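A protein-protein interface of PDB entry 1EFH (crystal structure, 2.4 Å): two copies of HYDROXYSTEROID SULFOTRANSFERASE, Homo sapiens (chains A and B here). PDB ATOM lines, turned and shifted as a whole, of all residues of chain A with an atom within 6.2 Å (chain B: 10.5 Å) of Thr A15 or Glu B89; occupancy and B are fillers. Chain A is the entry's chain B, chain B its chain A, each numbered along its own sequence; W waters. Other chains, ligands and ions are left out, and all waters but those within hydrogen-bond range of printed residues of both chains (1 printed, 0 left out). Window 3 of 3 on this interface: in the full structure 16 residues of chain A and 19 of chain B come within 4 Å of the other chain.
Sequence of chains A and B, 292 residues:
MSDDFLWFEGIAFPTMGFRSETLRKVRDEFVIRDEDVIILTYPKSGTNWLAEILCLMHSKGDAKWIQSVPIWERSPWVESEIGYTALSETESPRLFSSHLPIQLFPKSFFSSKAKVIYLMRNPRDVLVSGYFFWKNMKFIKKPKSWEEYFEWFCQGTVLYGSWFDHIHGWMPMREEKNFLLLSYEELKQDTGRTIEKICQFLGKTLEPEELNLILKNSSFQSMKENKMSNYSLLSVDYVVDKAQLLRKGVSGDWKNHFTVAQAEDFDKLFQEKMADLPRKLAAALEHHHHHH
No position is printed for both chains.
The guanidinium group (NH2) of Arg B33 sits at hydrogen-bond distance from the backbone carbonyl oxygen (O) of Thr B90 (2.7 Å).
The side-chain hydroxyl of Thr B85 sits at hydrogen-bond distance from the backbone carbonyl oxygen of Glu B81, 2.9 Å away.
The side-chain hydroxyl (OG1) of Thr B90 sits at hydrogen-bond distance from the backbone carbonyl oxygen (O) of Ala B86, 3.0 Å away.
The side-chain hydroxyl (OG1) of Thr A15 sits at hydrogen-bond distance from the backbone carbonyl oxygen (O) of Asp A4 (2.9 Å).
O of Phe A139 is in hydrogen-bond range of N of Thr A15, 2.5 Å away.
Among the printed residues, no Asp or Glu carboxylate lies within 4 Å of a Lys or Arg side-chain nitrogen of the other chain.
Thr A15 touches Glu B89.
CE of Met A16 touches CG2 of Thr B85 (3.5 Å).
SD of Met A16 touches CA of Ala B86, 3.6 Å away.
Met A16 touches Glu B89.
CA of Gly A17 touches CG2 of Thr B85, 3.98 Å away.
Lys A138 touches Thr B90 (NZ to CG2, 3.9 Å).
Phe A139 touches Glu B89.
N of Thr B90 touches CE2 of Phe A139, 3.8 Å away.
Water W1 bridges the backbone NH of Gly A17 (3.1 Å) and the backbone carbonyl oxygen of Thr B85 (3.2 Å).
Thr A15 touches just one residue of chain B: Glu B89 (3.7 Å).
Glu B89 touches just these residues of chain A: Thr A15 (3.7 Å), Met A16 (3.3 Å) and Phe A139 (3.7 Å).
No residue of chain B comes within 4 Å of Pro A14.
Printed residues of chain A within 4 Å of Thr B90: Lys A138 (3.9 Å) and Phe A139 (3.8 Å).
Printed residues of chain A within 4 Å of Ala B86: Met A16.
Of the printed residues of chain B, Lys A138 touches Thr B90 (3.9 Å).
Of the printed residues of chain B, Gly A17 touches Thr B85 (3.98 Å).
Printed residues of chain A within 4 Å of Thr B85: Met A16 (3.5 Å) and Gly A17 (3.98 Å).
Leu B95 touches none of the printed residues of chain A.
Glu B91 touches none of the printed residues of chain A.
The nearest residue of chain B that does not touch Thr A15 is Thr B90 (7.3 Å).
The nearest residue of chain A that does not touch Glu B89 is Gly A17 (4.9 Å).
The nearest printed residue of chain A that does not touch Thr B85 is Phe A18 (5.9 Å).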
ATOM      1  N   ASP A   4       4.778  21.978   3.035  1.00  0.00           N
ATOM      2  CA  ASP A   4       5.587  23.204   3.303  1.00  0.00           C
ATOM      3  C   ASP A   4       4.698  24.451   3.363  1.00  0.00           C
ATOM      4  O   ASP A   4       3.548  24.425   2.926  1.00  0.00           O
ATOM      5  CB  ASP A   4       6.661  23.367   2.219  1.00  0.00           C
ATOM      6  CG  ASP A   4       7.621  24.516   2.510  1.00  0.00           C
ATOM      7  OD1 ASP A   4       8.118  24.609   3.660  1.00  0.00           O
ATOM      8  OD2 ASP A   4       7.886  25.323   1.588  1.00  0.00           O
ATOM      9  N   PHE A   5       5.231  25.536   3.918  1.00  0.00           N
ATOM     10  CA  PHE A   5       4.484  26.786   4.033  1.00  0.00           C
ATOM     11  C   PHE A   5       4.649  27.659   2.791  1.00  0.00           C
ATOM     12  O   PHE A   5       5.507  27.411   1.946  1.00  0.00           O
ATOM     13  CB  PHE A   5       4.972  27.619   5.226  1.00  0.00           C
ATOM     14  CG  PHE A   5       4.883  26.925   6.553  1.00  0.00           C
ATOM     15  CD1 PHE A   5       6.042  26.501   7.208  1.00  0.00           C
ATOM     16  CD2 PHE A   5       3.653  26.750   7.185  1.00  0.00           C
ATOM     17  CE1 PHE A   5       5.980  25.917   8.479  1.00  0.00           C
ATOM     18  CE2 PHE A   5       3.577  26.167   8.455  1.00  0.00           C
ATOM     19  CZ  PHE A   5       4.748  25.750   9.104  1.00  0.00           C
ATOM     20  N   LEU A   6       3.807  28.682   2.695  1.00  0.00           N
ATOM     21  CA  LEU A   6       3.882  29.654   1.619  1.00  0.00           C
ATOM     22  C   LEU A   6       4.583  30.817   2.294  1.00  0.00           C
ATOM     23  O   LEU A   6       3.978  31.499   3.114  1.00  0.00           O
ATOM     24  CB  LEU A   6       2.494  30.103   1.182  1.00  0.00           C
ATOM     25  CG  LEU A   6       2.459  31.502   0.544  1.00  0.00           C
ATOM     26  CD1 LEU A   6       3.373  31.560  -0.673  1.00  0.00           C
ATOM     27  CD2 LEU A   6       1.033  31.847   0.153  1.00  0.00           C
ATOM     28  N   PHE A  13       2.555  31.168   5.783  1.00  0.00           N
ATOM     29  CA  PHE A  13       1.110  31.155   5.559  1.00  0.00           C
ATOM     30  C   PHE A  13       0.711  29.792   5.018  1.00  0.00           C
ATOM     31  O   PHE A  13       1.568  28.992   4.633  1.00  0.00           O
ATOM     32  CB  PHE A  13       0.691  32.215   4.530  1.00  0.00           C
ATOM     33  CG  PHE A  13       0.866  33.626   4.996  1.00  0.00           C
ATOM     34  CD1 PHE A  13       2.127  34.215   5.022  1.00  0.00           C
ATOM     35  CD2 PHE A  13      -0.235  34.377   5.395  1.00  0.00           C
ATOM     36  CE1 PHE A  13       2.288  35.533   5.436  1.00  0.00           C
ATOM     37  CE2 PHE A  13      -0.085  35.696   5.812  1.00  0.00           C
ATOM     38  CZ  PHE A  13       1.177  36.277   5.831  1.00  0.00           C
ATOM     39  N   PRO A  14      -0.600  29.500   4.989  1.00  0.00           N
ATOM     40  CA  PRO A  14      -1.049  28.206   4.469  1.00  0.00           C
ATOM     41  C   PRO A  14      -0.808  28.128   2.952  1.00  0.00           C
ATOM     42  O   PRO A  14      -0.802  29.151   2.249  1.00  0.00           O
ATOM     43  CB  PRO A  14      -2.535  28.193   4.818  1.00  0.00           C
ATOM     44  CG  PRO A  14      -2.613  29.069   6.013  1.00  0.00           C
ATOM     45  CD  PRO A  14      -1.718  30.209   5.631  1.00  0.00           C
ATOM     46  N   THR A  15      -0.608  26.910   2.461  1.00  0.00           N
ATOM     47  CA  THR A  15      -0.357  26.679   1.047  1.00  0.00           C
ATOM     48  C   THR A  15      -1.547  27.025   0.167  1.00  0.00           C
ATOM     49  O   THR A  15      -1.373  27.587  -0.913  1.00  0.00           O
ATOM     50  CB  THR A  15       0.062  25.217   0.805  1.00  0.00           C
ATOM     51  OG1 THR A  15       1.470  25.094   1.048  1.00  0.00           O
ATOM     52  CG2 THR A  15      -0.254  24.779  -0.624  1.00  0.00           C
ATOM     53  N   MET A  16      -2.755  26.700   0.617  1.00  0.00           N
ATOM     54  CA  MET A  16      -3.931  27.011  -0.183  1.00  0.00           C
ATOM     55  C   MET A  16      -4.749  28.126   0.453  1.00  0.00           C
ATOM     56  O   MET A  16      -4.771  28.264   1.672  1.00  0.00           O
ATOM     57  CB  MET A  16      -4.813  25.776  -0.353  1.00  0.00           C
ATOM     58  CG  MET A  16      -5.879  25.645   0.703  1.00  0.00           C
ATOM     59  SD  MET A  16      -7.530  25.562  -0.016  1.00  0.00           S
ATOM     60  CE  MET A  16      -8.079  27.252   0.121  1.00  0.00           C
ATOM     61  N   GLY A  17      -5.418  28.914  -0.383  1.00  0.00           N
ATOM     62  CA  GLY A  17      -6.241  29.999   0.114  1.00  0.00           C
ATOM     63  C   GLY A  17      -5.550  31.346   0.189  1.00  0.00           C
ATOM     64  O   GLY A  17      -6.203  32.359   0.437  1.00  0.00           O
ATOM     65  N   PHE A  18      -4.236  31.365  -0.019  1.00  0.00           N
ATOM     66  CA  PHE A  18      -3.477  32.607   0.043  1.00  0.00           C
ATOM     67  C   PHE A  18      -2.482  32.738  -1.098  1.00  0.00           C
ATOM     68  O   PHE A  18      -1.791  31.780  -1.443  1.00  0.00           O
ATOM     69  CB  PHE A  18      -2.723  32.710   1.376  1.00  0.00           C
ATOM     70  CG  PHE A  18      -3.602  32.550   2.589  1.00  0.00           C
ATOM     71  CD1 PHE A  18      -4.011  31.285   3.009  1.00  0.00           C
ATOM     72  CD2 PHE A  18      -4.049  33.669   3.294  1.00  0.00           C
ATOM     73  CE1 PHE A  18      -4.857  31.137   4.111  1.00  0.00           C
ATOM     74  CE2 PHE A  18      -4.896  33.529   4.396  1.00  0.00           C
ATOM     75  CZ  PHE A  18      -5.301  32.261   4.806  1.00  0.00           C
ATOM     76  N   LYS A 138      -4.160  20.208   6.431  1.00  0.00           N
ATOM     77  CA  LYS A 138      -3.463  20.096   5.159  1.00  0.00           C
ATOM     78  C   LYS A 138      -3.052  21.501   4.727  1.00  0.00           C
ATOM     79  O   LYS A 138      -3.503  22.494   5.307  1.00  0.00           O
ATOM     80  CB  LYS A 138      -4.396  19.486   4.103  1.00  0.00           C
ATOM     81  CG  LYS A 138      -4.897  18.078   4.437  1.00  0.00           C
ATOM     82  CD  LYS A 138      -6.117  17.674   3.598  1.00  0.00           C
ATOM     83  CE  LYS A 138      -5.811  17.634   2.105  1.00  0.00           C
ATOM     84  NZ  LYS A 138      -6.990  17.201   1.299  1.00  0.00           N
ATOM     85  N   PHE A 139      -2.187  21.575   3.722  1.00  0.00           N
ATOM     86  CA  PHE A 139      -1.723  22.850   3.180  1.00  0.00           C
ATOM     87  C   PHE A 139      -0.759  23.620   4.082  1.00  0.00           C
ATOM     88  O   PHE A 139      -0.497  24.801   3.851  1.00  0.00           O
ATOM     89  CB  PHE A 139      -2.929  23.731   2.831  1.00  0.00           C
ATOM     90  CG  PHE A 139      -3.961  23.034   1.981  1.00  0.00           C
ATOM     91  CD1 PHE A 139      -5.292  22.972   2.392  1.00  0.00           C
ATOM     92  CD2 PHE A 139      -3.601  22.435   0.776  1.00  0.00           C
ATOM     93  CE1 PHE A 139      -6.249  22.323   1.616  1.00  0.00           C
ATOM     94  CE2 PHE A 139      -4.549  21.784  -0.008  1.00  0.00           C
ATOM     95  CZ  PHE A 139      -5.878  21.728   0.412  1.00  0.00           C
ATOM     96  N   ILE A 140      -0.237  22.955   5.108  1.00  0.00           N
ATOM     97  CA  ILE A 140       0.719  23.578   6.021  1.00  0.00           C
ATOM     98  C   ILE A 140       1.735  22.529   6.458  1.00  0.00           C
ATOM     99  O   ILE A 140       1.430  21.338   6.475  1.00  0.00           O
ATOM    100  CB  ILE A 140       0.030  24.151   7.281  1.00  0.00           C
ATOM    101  CG1 ILE A 140      -0.534  23.014   8.131  1.00  0.00           C
ATOM    102  CG2 ILE A 140      -1.073  25.123   6.875  1.00  0.00           C
ATOM    103  CD1 ILE A 140      -1.133  23.470   9.439  1.00  0.00           C
ATOM    104  N   LYS B  25     -11.394  31.245 -15.808  1.00  0.00           N
ATOM    105  CA  LYS B  25     -10.225  30.463 -15.416  1.00  0.00           C
ATOM    106  C   LYS B  25     -10.580  28.989 -15.284  1.00  0.00           C
ATOM    107  O   LYS B  25      -9.794  28.110 -15.667  1.00  0.00           O
ATOM    108  CB  LYS B  25      -9.638  30.996 -14.099  1.00  0.00           C
ATOM    109  CG  LYS B  25      -8.613  32.124 -14.282  1.00  0.00           C
ATOM    110  CD  LYS B  25      -8.605  33.098 -13.102  1.00  0.00           C
ATOM    111  CE  LYS B  25      -8.429  32.396 -11.765  1.00  0.00           C
ATOM    112  NZ  LYS B  25      -8.645  33.320 -10.614  1.00  0.00           N
ATOM    113  N   PHE B  30      -8.027  25.952 -15.271  1.00  0.00           N
ATOM    114  CA  PHE B  30      -8.078  24.908 -14.254  1.00  0.00           C
ATOM    115  C   PHE B  30      -7.503  23.593 -14.781  1.00  0.00           C
ATOM    116  O   PHE B  30      -7.894  23.125 -15.849  1.00  0.00           O
ATOM    117  CB  PHE B  30      -9.520  24.686 -13.815  1.00  0.00           C
ATOM    118  CG  PHE B  30      -9.657  23.812 -12.604  1.00  0.00           C
ATOM    119  CD1 PHE B  30      -9.571  24.356 -11.328  1.00  0.00           C
ATOM    120  CD2 PHE B  30      -9.881  22.444 -12.738  1.00  0.00           C
ATOM    121  CE1 PHE B  30      -9.711  23.551 -10.198  1.00  0.00           C
ATOM    122  CE2 PHE B  30     -10.021  21.630 -11.616  1.00  0.00           C
ATOM    123  CZ  PHE B  30      -9.938  22.186 -10.344  1.00  0.00           C
ATOM    124  N   VAL B  31      -6.581  22.995 -14.031  1.00  0.00           N
ATOM    125  CA  VAL B  31      -5.966  21.733 -14.445  1.00  0.00           C
ATOM    126  C   VAL B  31      -6.743  20.516 -13.951  1.00  0.00           C
ATOM    127  O   VAL B  31      -7.013  20.379 -12.768  1.00  0.00           O
ATOM    128  CB  VAL B  31      -4.506  21.630 -13.935  1.00  0.00           C
ATOM    129  CG1 VAL B  31      -3.883  20.289 -14.338  1.00  0.00           C
ATOM    130  CG2 VAL B  31      -3.695  22.773 -14.499  1.00  0.00           C
ATOM    131  N   ARG B  33      -6.874  16.451 -13.485  1.00  0.00           N
ATOM    132  CA  ARG B  33      -5.924  15.351 -13.334  1.00  0.00           C
ATOM    133  C   ARG B  33      -6.586  14.001 -13.580  1.00  0.00           C
ATOM    134  O   ARG B  33      -7.751  13.803 -13.230  1.00  0.00           O
ATOM    135  CB  ARG B  33      -5.307  15.397 -11.932  1.00  0.00           C
ATOM    136  CG  ARG B  33      -4.892  16.809 -11.508  1.00  0.00           C
ATOM    137  CD  ARG B  33      -3.783  16.802 -10.461  1.00  0.00           C
ATOM    138  NE  ARG B  33      -4.270  16.643  -9.095  1.00  0.00           N
ATOM    139  CZ  ARG B  33      -4.485  17.649  -8.252  1.00  0.00           C
ATOM    140  NH1 ARG B  33      -4.260  18.900  -8.635  1.00  0.00           N
ATOM    141  NH2 ARG B  33      -4.912  17.398  -7.021  1.00  0.00           N
ATOM    142  N   ASP B  36      -8.815  12.440 -10.884  1.00  0.00           N
ATOM    143  CA  ASP B  36     -10.011  13.141 -10.430  1.00  0.00           C
ATOM    144  C   ASP B  36     -11.265  12.307 -10.743  1.00  0.00           C
ATOM    145  O   ASP B  36     -11.312  11.574 -11.737  1.00  0.00           O
ATOM    146  CB  ASP B  36     -10.132  14.493 -11.140  1.00  0.00           C
ATOM    147  CG  ASP B  36      -9.003  15.444 -10.796  1.00  0.00           C
ATOM    148  OD1 ASP B  36      -8.759  16.386 -11.585  1.00  0.00           O
ATOM    149  OD2 ASP B  36      -8.367  15.251  -9.736  1.00  0.00           O
ATOM    150  N   PRO B  76     -16.264  19.481  -3.356  1.00  0.00           N
ATOM    151  CA  PRO B  76     -16.432  20.886  -3.727  1.00  0.00           C
ATOM    152  C   PRO B  76     -17.126  21.114  -5.069  1.00  0.00           C
ATOM    153  O   PRO B  76     -17.106  20.267  -5.959  1.00  0.00           O
ATOM    154  CB  PRO B  76     -14.995  21.423  -3.732  1.00  0.00           C
ATOM    155  CG  PRO B  76     -14.295  20.540  -2.767  1.00  0.00           C
ATOM    156  CD  PRO B  76     -14.844  19.176  -3.113  1.00  0.00           C
ATOM    157  N   VAL B  78     -16.602  22.902  -7.991  1.00  0.00           N
ATOM    158  CA  VAL B  78     -15.475  23.509  -8.701  1.00  0.00           C
ATOM    159  C   VAL B  78     -15.607  24.912  -9.301  1.00  0.00           C
ATOM    160  O   VAL B  78     -14.662  25.697  -9.221  1.00  0.00           O
ATOM    161  CB  VAL B  78     -14.919  22.544  -9.797  1.00  0.00           C
ATOM    162  CG1 VAL B  78     -15.881  22.444 -10.955  1.00  0.00           C
ATOM    163  CG2 VAL B  78     -13.557  23.019 -10.273  1.00  0.00           C
ATOM    164  N   GLU B  81     -16.530  29.994  -6.065  1.00  0.00           N
ATOM    165  CA  GLU B  81     -15.313  30.593  -5.514  1.00  0.00           C
ATOM    166  C   GLU B  81     -14.591  29.663  -4.537  1.00  0.00           C
ATOM    167  O   GLU B  81     -13.408  29.379  -4.698  1.00  0.00           O
ATOM    168  CB  GLU B  81     -15.634  31.918  -4.808  1.00  0.00           C
ATOM    169  CG  GLU B  81     -15.787  33.096  -5.746  1.00  0.00           C
ATOM    170  CD  GLU B  81     -14.508  33.378  -6.515  1.00  0.00           C
ATOM    171  OE1 GLU B  81     -13.515  33.827  -5.896  1.00  0.00           O
ATOM    172  OE2 GLU B  81     -14.494  33.136  -7.738  1.00  0.00           O
ATOM    173  N   ILE B  82     -15.315  29.196  -3.527  1.00  0.00           N
ATOM    174  CA  ILE B  82     -14.757  28.309  -2.520  1.00  0.00           C
ATOM    175  C   ILE B  82     -14.205  27.014  -3.108  1.00  0.00           C
ATOM    176  O   ILE B  82     -13.119  26.564  -2.725  1.00  0.00           O
ATOM    177  CB  ILE B  82     -15.826  27.976  -1.456  1.00  0.00           C
ATOM    178  CG1 ILE B  82     -16.183  29.250  -0.685  1.00  0.00           C
ATOM    179  CG2 ILE B  82     -15.321  26.901  -0.503  1.00  0.00           C
ATOM    180  CD1 ILE B  82     -17.450  29.128   0.129  1.00  0.00           C
ATOM    181  N   GLY B  83     -14.949  26.423  -4.038  1.00  0.00           N
ATOM    182  CA  GLY B  83     -14.516  25.179  -4.648  1.00  0.00           C
ATOM    183  C   GLY B  83     -13.271  25.320  -5.502  1.00  0.00           C
ATOM    184  O   GLY B  83     -12.334  24.515  -5.408  1.00  0.00           O
ATOM    185  N   TYR B  84     -13.269  26.337  -6.357  1.00  0.00           N
ATOM    186  CA  TYR B  84     -12.133  26.608  -7.230  1.00  0.00           C
ATOM    187  C   TYR B  84     -10.872  26.787  -6.385  1.00  0.00           C
ATOM    188  O   TYR B  84      -9.850  26.144  -6.611  1.00  0.00           O
ATOM    189  CB  TYR B  84     -12.393  27.884  -8.033  1.00  0.00           C
ATOM    190  CG  TYR B  84     -11.211  28.344  -8.847  1.00  0.00           C
ATOM    191  CD1 TYR B  84     -10.902  27.750 -10.072  1.00  0.00           C
ATOM    192  CD2 TYR B  84     -10.390  29.377  -8.388  1.00  0.00           C
ATOM    193  CE1 TYR B  84      -9.810  28.174 -10.824  1.00  0.00           C
ATOM    194  CE2 TYR B  84      -9.290  29.808  -9.131  1.00  0.00           C
ATOM    195  CZ  TYR B  84      -9.008  29.206 -10.344  1.00  0.00           C
ATOM    196  OH  TYR B  84      -7.927  29.636 -11.071  1.00  0.00           O
ATOM    197  N   THR B  85     -10.968  27.670  -5.402  1.00  0.00           N
ATOM    198  CA  THR B  85      -9.863  27.963  -4.514  1.00  0.00           C
ATOM    199  C   THR B  85      -9.359  26.709  -3.826  1.00  0.00           C
ATOM    200  O   THR B  85      -8.158  26.456  -3.791  1.00  0.00           O
ATOM    201  CB  THR B  85     -10.290  28.978  -3.456  1.00  0.00           C
ATOM    202  OG1 THR B  85     -10.715  30.175  -4.110  1.00  0.00           O
ATOM    203  CG2 THR B  85      -9.139  29.297  -2.524  1.00  0.00           C
ATOM    204  N   ALA B  86     -10.280  25.919  -3.286  1.00  0.00           N
ATOM    205  CA  ALA B  86      -9.910  24.695  -2.591  1.00  0.00           C
ATOM    206  C   ALA B  86      -9.240  23.682  -3.512  1.00  0.00           C
ATOM    207  O   ALA B  86      -8.106  23.263  -3.265  1.00  0.00           O
ATOM    208  CB  ALA B  86     -11.141  24.072  -1.941  1.00  0.00           C
ATOM    209  N   LEU B  87      -9.949  23.296  -4.572  1.00  0.00           N
ATOM    210  CA  LEU B  87      -9.450  22.308  -5.527  1.00  0.00           C
ATOM    211  C   LEU B  87      -8.111  22.658  -6.164  1.00  0.00           C
ATOM    212  O   LEU B  87      -7.290  21.776  -6.405  1.00  0.00           O
ATOM    213  CB  LEU B  87     -10.483  22.066  -6.636  1.00  0.00           C
ATOM    214  CG  LEU B  87     -11.689  21.137  -6.439  1.00  0.00           C
ATOM    215  CD1 LEU B  87     -11.834  20.706  -5.001  1.00  0.00           C
ATOM    216  CD2 LEU B  87     -12.940  21.855  -6.916  1.00  0.00           C
ATOM    217  N   SER B  88      -7.891  23.937  -6.448  1.00  0.00           N
ATOM    218  CA  SER B  88      -6.638  24.358  -7.070  1.00  0.00           C
ATOM    219  C   SER B  88      -5.415  23.881  -6.297  1.00  0.00           C
ATOM    220  O   SER B  88      -4.299  23.948  -6.801  1.00  0.00           O
ATOM    221  CB  SER B  88      -6.584  25.884  -7.201  1.00  0.00           C
ATOM    222  OG  SER B  88      -7.538  26.375  -8.132  1.00  0.00           O
ATOM    223  N   GLU B  89      -5.624  23.389  -5.080  1.00  0.00           N
ATOM    224  CA  GLU B  89      -4.514  22.929  -4.253  1.00  0.00           C
ATOM    225  C   GLU B  89      -4.674  21.525  -3.684  1.00  0.00           C
ATOM    226  O   GLU B  89      -3.679  20.850  -3.433  1.00  0.00           O
ATOM    227  CB  GLU B  89      -4.296  23.902  -3.092  1.00  0.00           C
ATOM    228  CG  GLU B  89      -4.068  25.337  -3.519  1.00  0.00           C
ATOM    229  CD  GLU B  89      -2.844  25.488  -4.391  1.00  0.00           C
ATOM    230  OE1 GLU B  89      -1.763  25.006  -3.975  1.00  0.00           O
ATOM    231  OE2 GLU B  89      -2.966  26.092  -5.483  1.00  0.00           O
ATOM    232  N   THR B  90      -5.916  21.097  -3.466  1.00  0.00           N
ATOM    233  CA  THR B  90      -6.194  19.778  -2.901  1.00  0.00           C
ATOM    234  C   THR B  90      -5.344  18.690  -3.537  1.00  0.00           C
ATOM    235  O   THR B  90      -4.998  18.774  -4.716  1.00  0.00           O
ATOM    236  CB  THR B  90      -7.671  19.404  -3.062  1.00  0.00           C
ATOM    237  OG1 THR B  90      -8.488  20.434  -2.492  1.00  0.00           O
ATOM    238  CG2 THR B  90      -7.961  18.088  -2.358  1.00  0.00           C
ATOM    239  N   GLU B  91      -5.011  17.669  -2.752  1.00  0.00           N
ATOM    240  CA  GLU B  91      -4.180  16.561  -3.224  1.00  0.00           C
ATOM    241  C   GLU B  91      -4.976  15.422  -3.862  1.00  0.00           C
ATOM    242  O   GLU B  91      -6.098  15.120  -3.453  1.00  0.00           O
ATOM    243  CB  GLU B  91      -3.328  16.020  -2.064  1.00  0.00           C
ATOM    244  N   SER B  92      -4.388  14.789  -4.871  1.00  0.00           N
ATOM    245  CA  SER B  92      -5.042  13.675  -5.538  1.00  0.00           C
ATOM    246  C   SER B  92      -5.166  12.524  -4.551  1.00  0.00           C
ATOM    247  O   SER B  92      -4.347  12.374  -3.645  1.00  0.00           O
ATOM    248  CB  SER B  92      -4.227  13.207  -6.745  1.00  0.00           C
ATOM    249  OG  SER B  92      -4.118  14.221  -7.726  1.00  0.00           O
ATOM    250  N   PRO B  93      -6.211  11.705  -4.702  1.00  0.00           N
ATOM    251  CA  PRO B  93      -7.207  11.894  -5.760  1.00  0.00           C
ATOM    252  C   PRO B  93      -8.286  12.886  -5.321  1.00  0.00           C
ATOM    253  O   PRO B  93      -8.747  12.852  -4.180  1.00  0.00           O
ATOM    254  CB  PRO B  93      -7.753  10.483  -5.971  1.00  0.00           C
ATOM    255  CG  PRO B  93      -7.706   9.913  -4.579  1.00  0.00           C
ATOM    256  CD  PRO B  93      -6.350  10.381  -4.070  1.00  0.00           C
ATOM    257  N   ARG B  94      -8.676  13.773  -6.226  1.00  0.00           N
ATOM    258  CA  ARG B  94      -9.706  14.756  -5.920  1.00  0.00           C
ATOM    259  C   ARG B  94     -11.093  14.254  -6.316  1.00  0.00           C
ATOM    260  O   ARG B  94     -11.234  13.505  -7.280  1.00  0.00           O
ATOM    261  CB  ARG B  94      -9.442  16.063  -6.665  1.00  0.00           C
ATOM    262  CG  ARG B  94      -8.109  16.719  -6.375  1.00  0.00           C
ATOM    263  CD  ARG B  94      -8.005  18.075  -7.066  1.00  0.00           C
ATOM    264  NE  ARG B  94      -8.097  17.987  -8.524  1.00  0.00           N
ATOM    265  CZ  ARG B  94      -7.908  19.017  -9.342  1.00  0.00           C
ATOM    266  NH1 ARG B  94      -7.623  20.213  -8.845  1.00  0.00           N
ATOM    267  NH2 ARG B  94      -7.983  18.858 -10.658  1.00  0.00           N
ATOM    268  N   LEU B  95     -12.102  14.663  -5.548  1.00  0.00           N
ATOM    269  CA  LEU B  95     -13.502  14.338  -5.818  1.00  0.00           C
ATOM    270  C   LEU B  95     -14.230  15.671  -5.805  1.00  0.00           C
ATOM    271  O   LEU B  95     -14.173  16.389  -4.811  1.00  0.00           O
ATOM    272  CB  LEU B  95     -14.116  13.455  -4.722  1.00  0.00           C
ATOM    273  CG  LEU B  95     -15.664  13.425  -4.739  1.00  0.00           C
ATOM    274  CD1 LEU B  95     -16.160  12.690  -5.984  1.00  0.00           C
ATOM    275  CD2 LEU B  95     -16.204  12.742  -3.489  1.00  0.00           C
ATOM    276  N   PHE B  96     -14.877  16.032  -6.905  1.00  0.00           N
ATOM    277  CA  PHE B  96     -15.627  17.281  -6.932  1.00  0.00           C
ATOM    278  C   PHE B  96     -16.813  17.204  -7.889  1.00  0.00           C
ATOM    279  O   PHE B  96     -16.963  16.223  -8.615  1.00  0.00           O
ATOM    280  CB  PHE B  96     -14.707  18.479  -7.243  1.00  0.00           C
ATOM    281  CG  PHE B  96     -13.922  18.363  -8.527  1.00  0.00           C
ATOM    282  CD1 PHE B  96     -14.405  18.923  -9.710  1.00  0.00           C
ATOM    283  CD2 PHE B  96     -12.666  17.744  -8.541  1.00  0.00           C
ATOM    284  CE1 PHE B  96     -13.650  18.874 -10.887  1.00  0.00           C
ATOM    285  CE2 PHE B  96     -11.906  17.691  -9.712  1.00  0.00           C
ATOM    286  CZ  PHE B  96     -12.402  18.259 -10.885  1.00  0.00           C
HETATM  287  O   HOH W   1      -5.427  28.123  -3.356  1.00  0.00           O
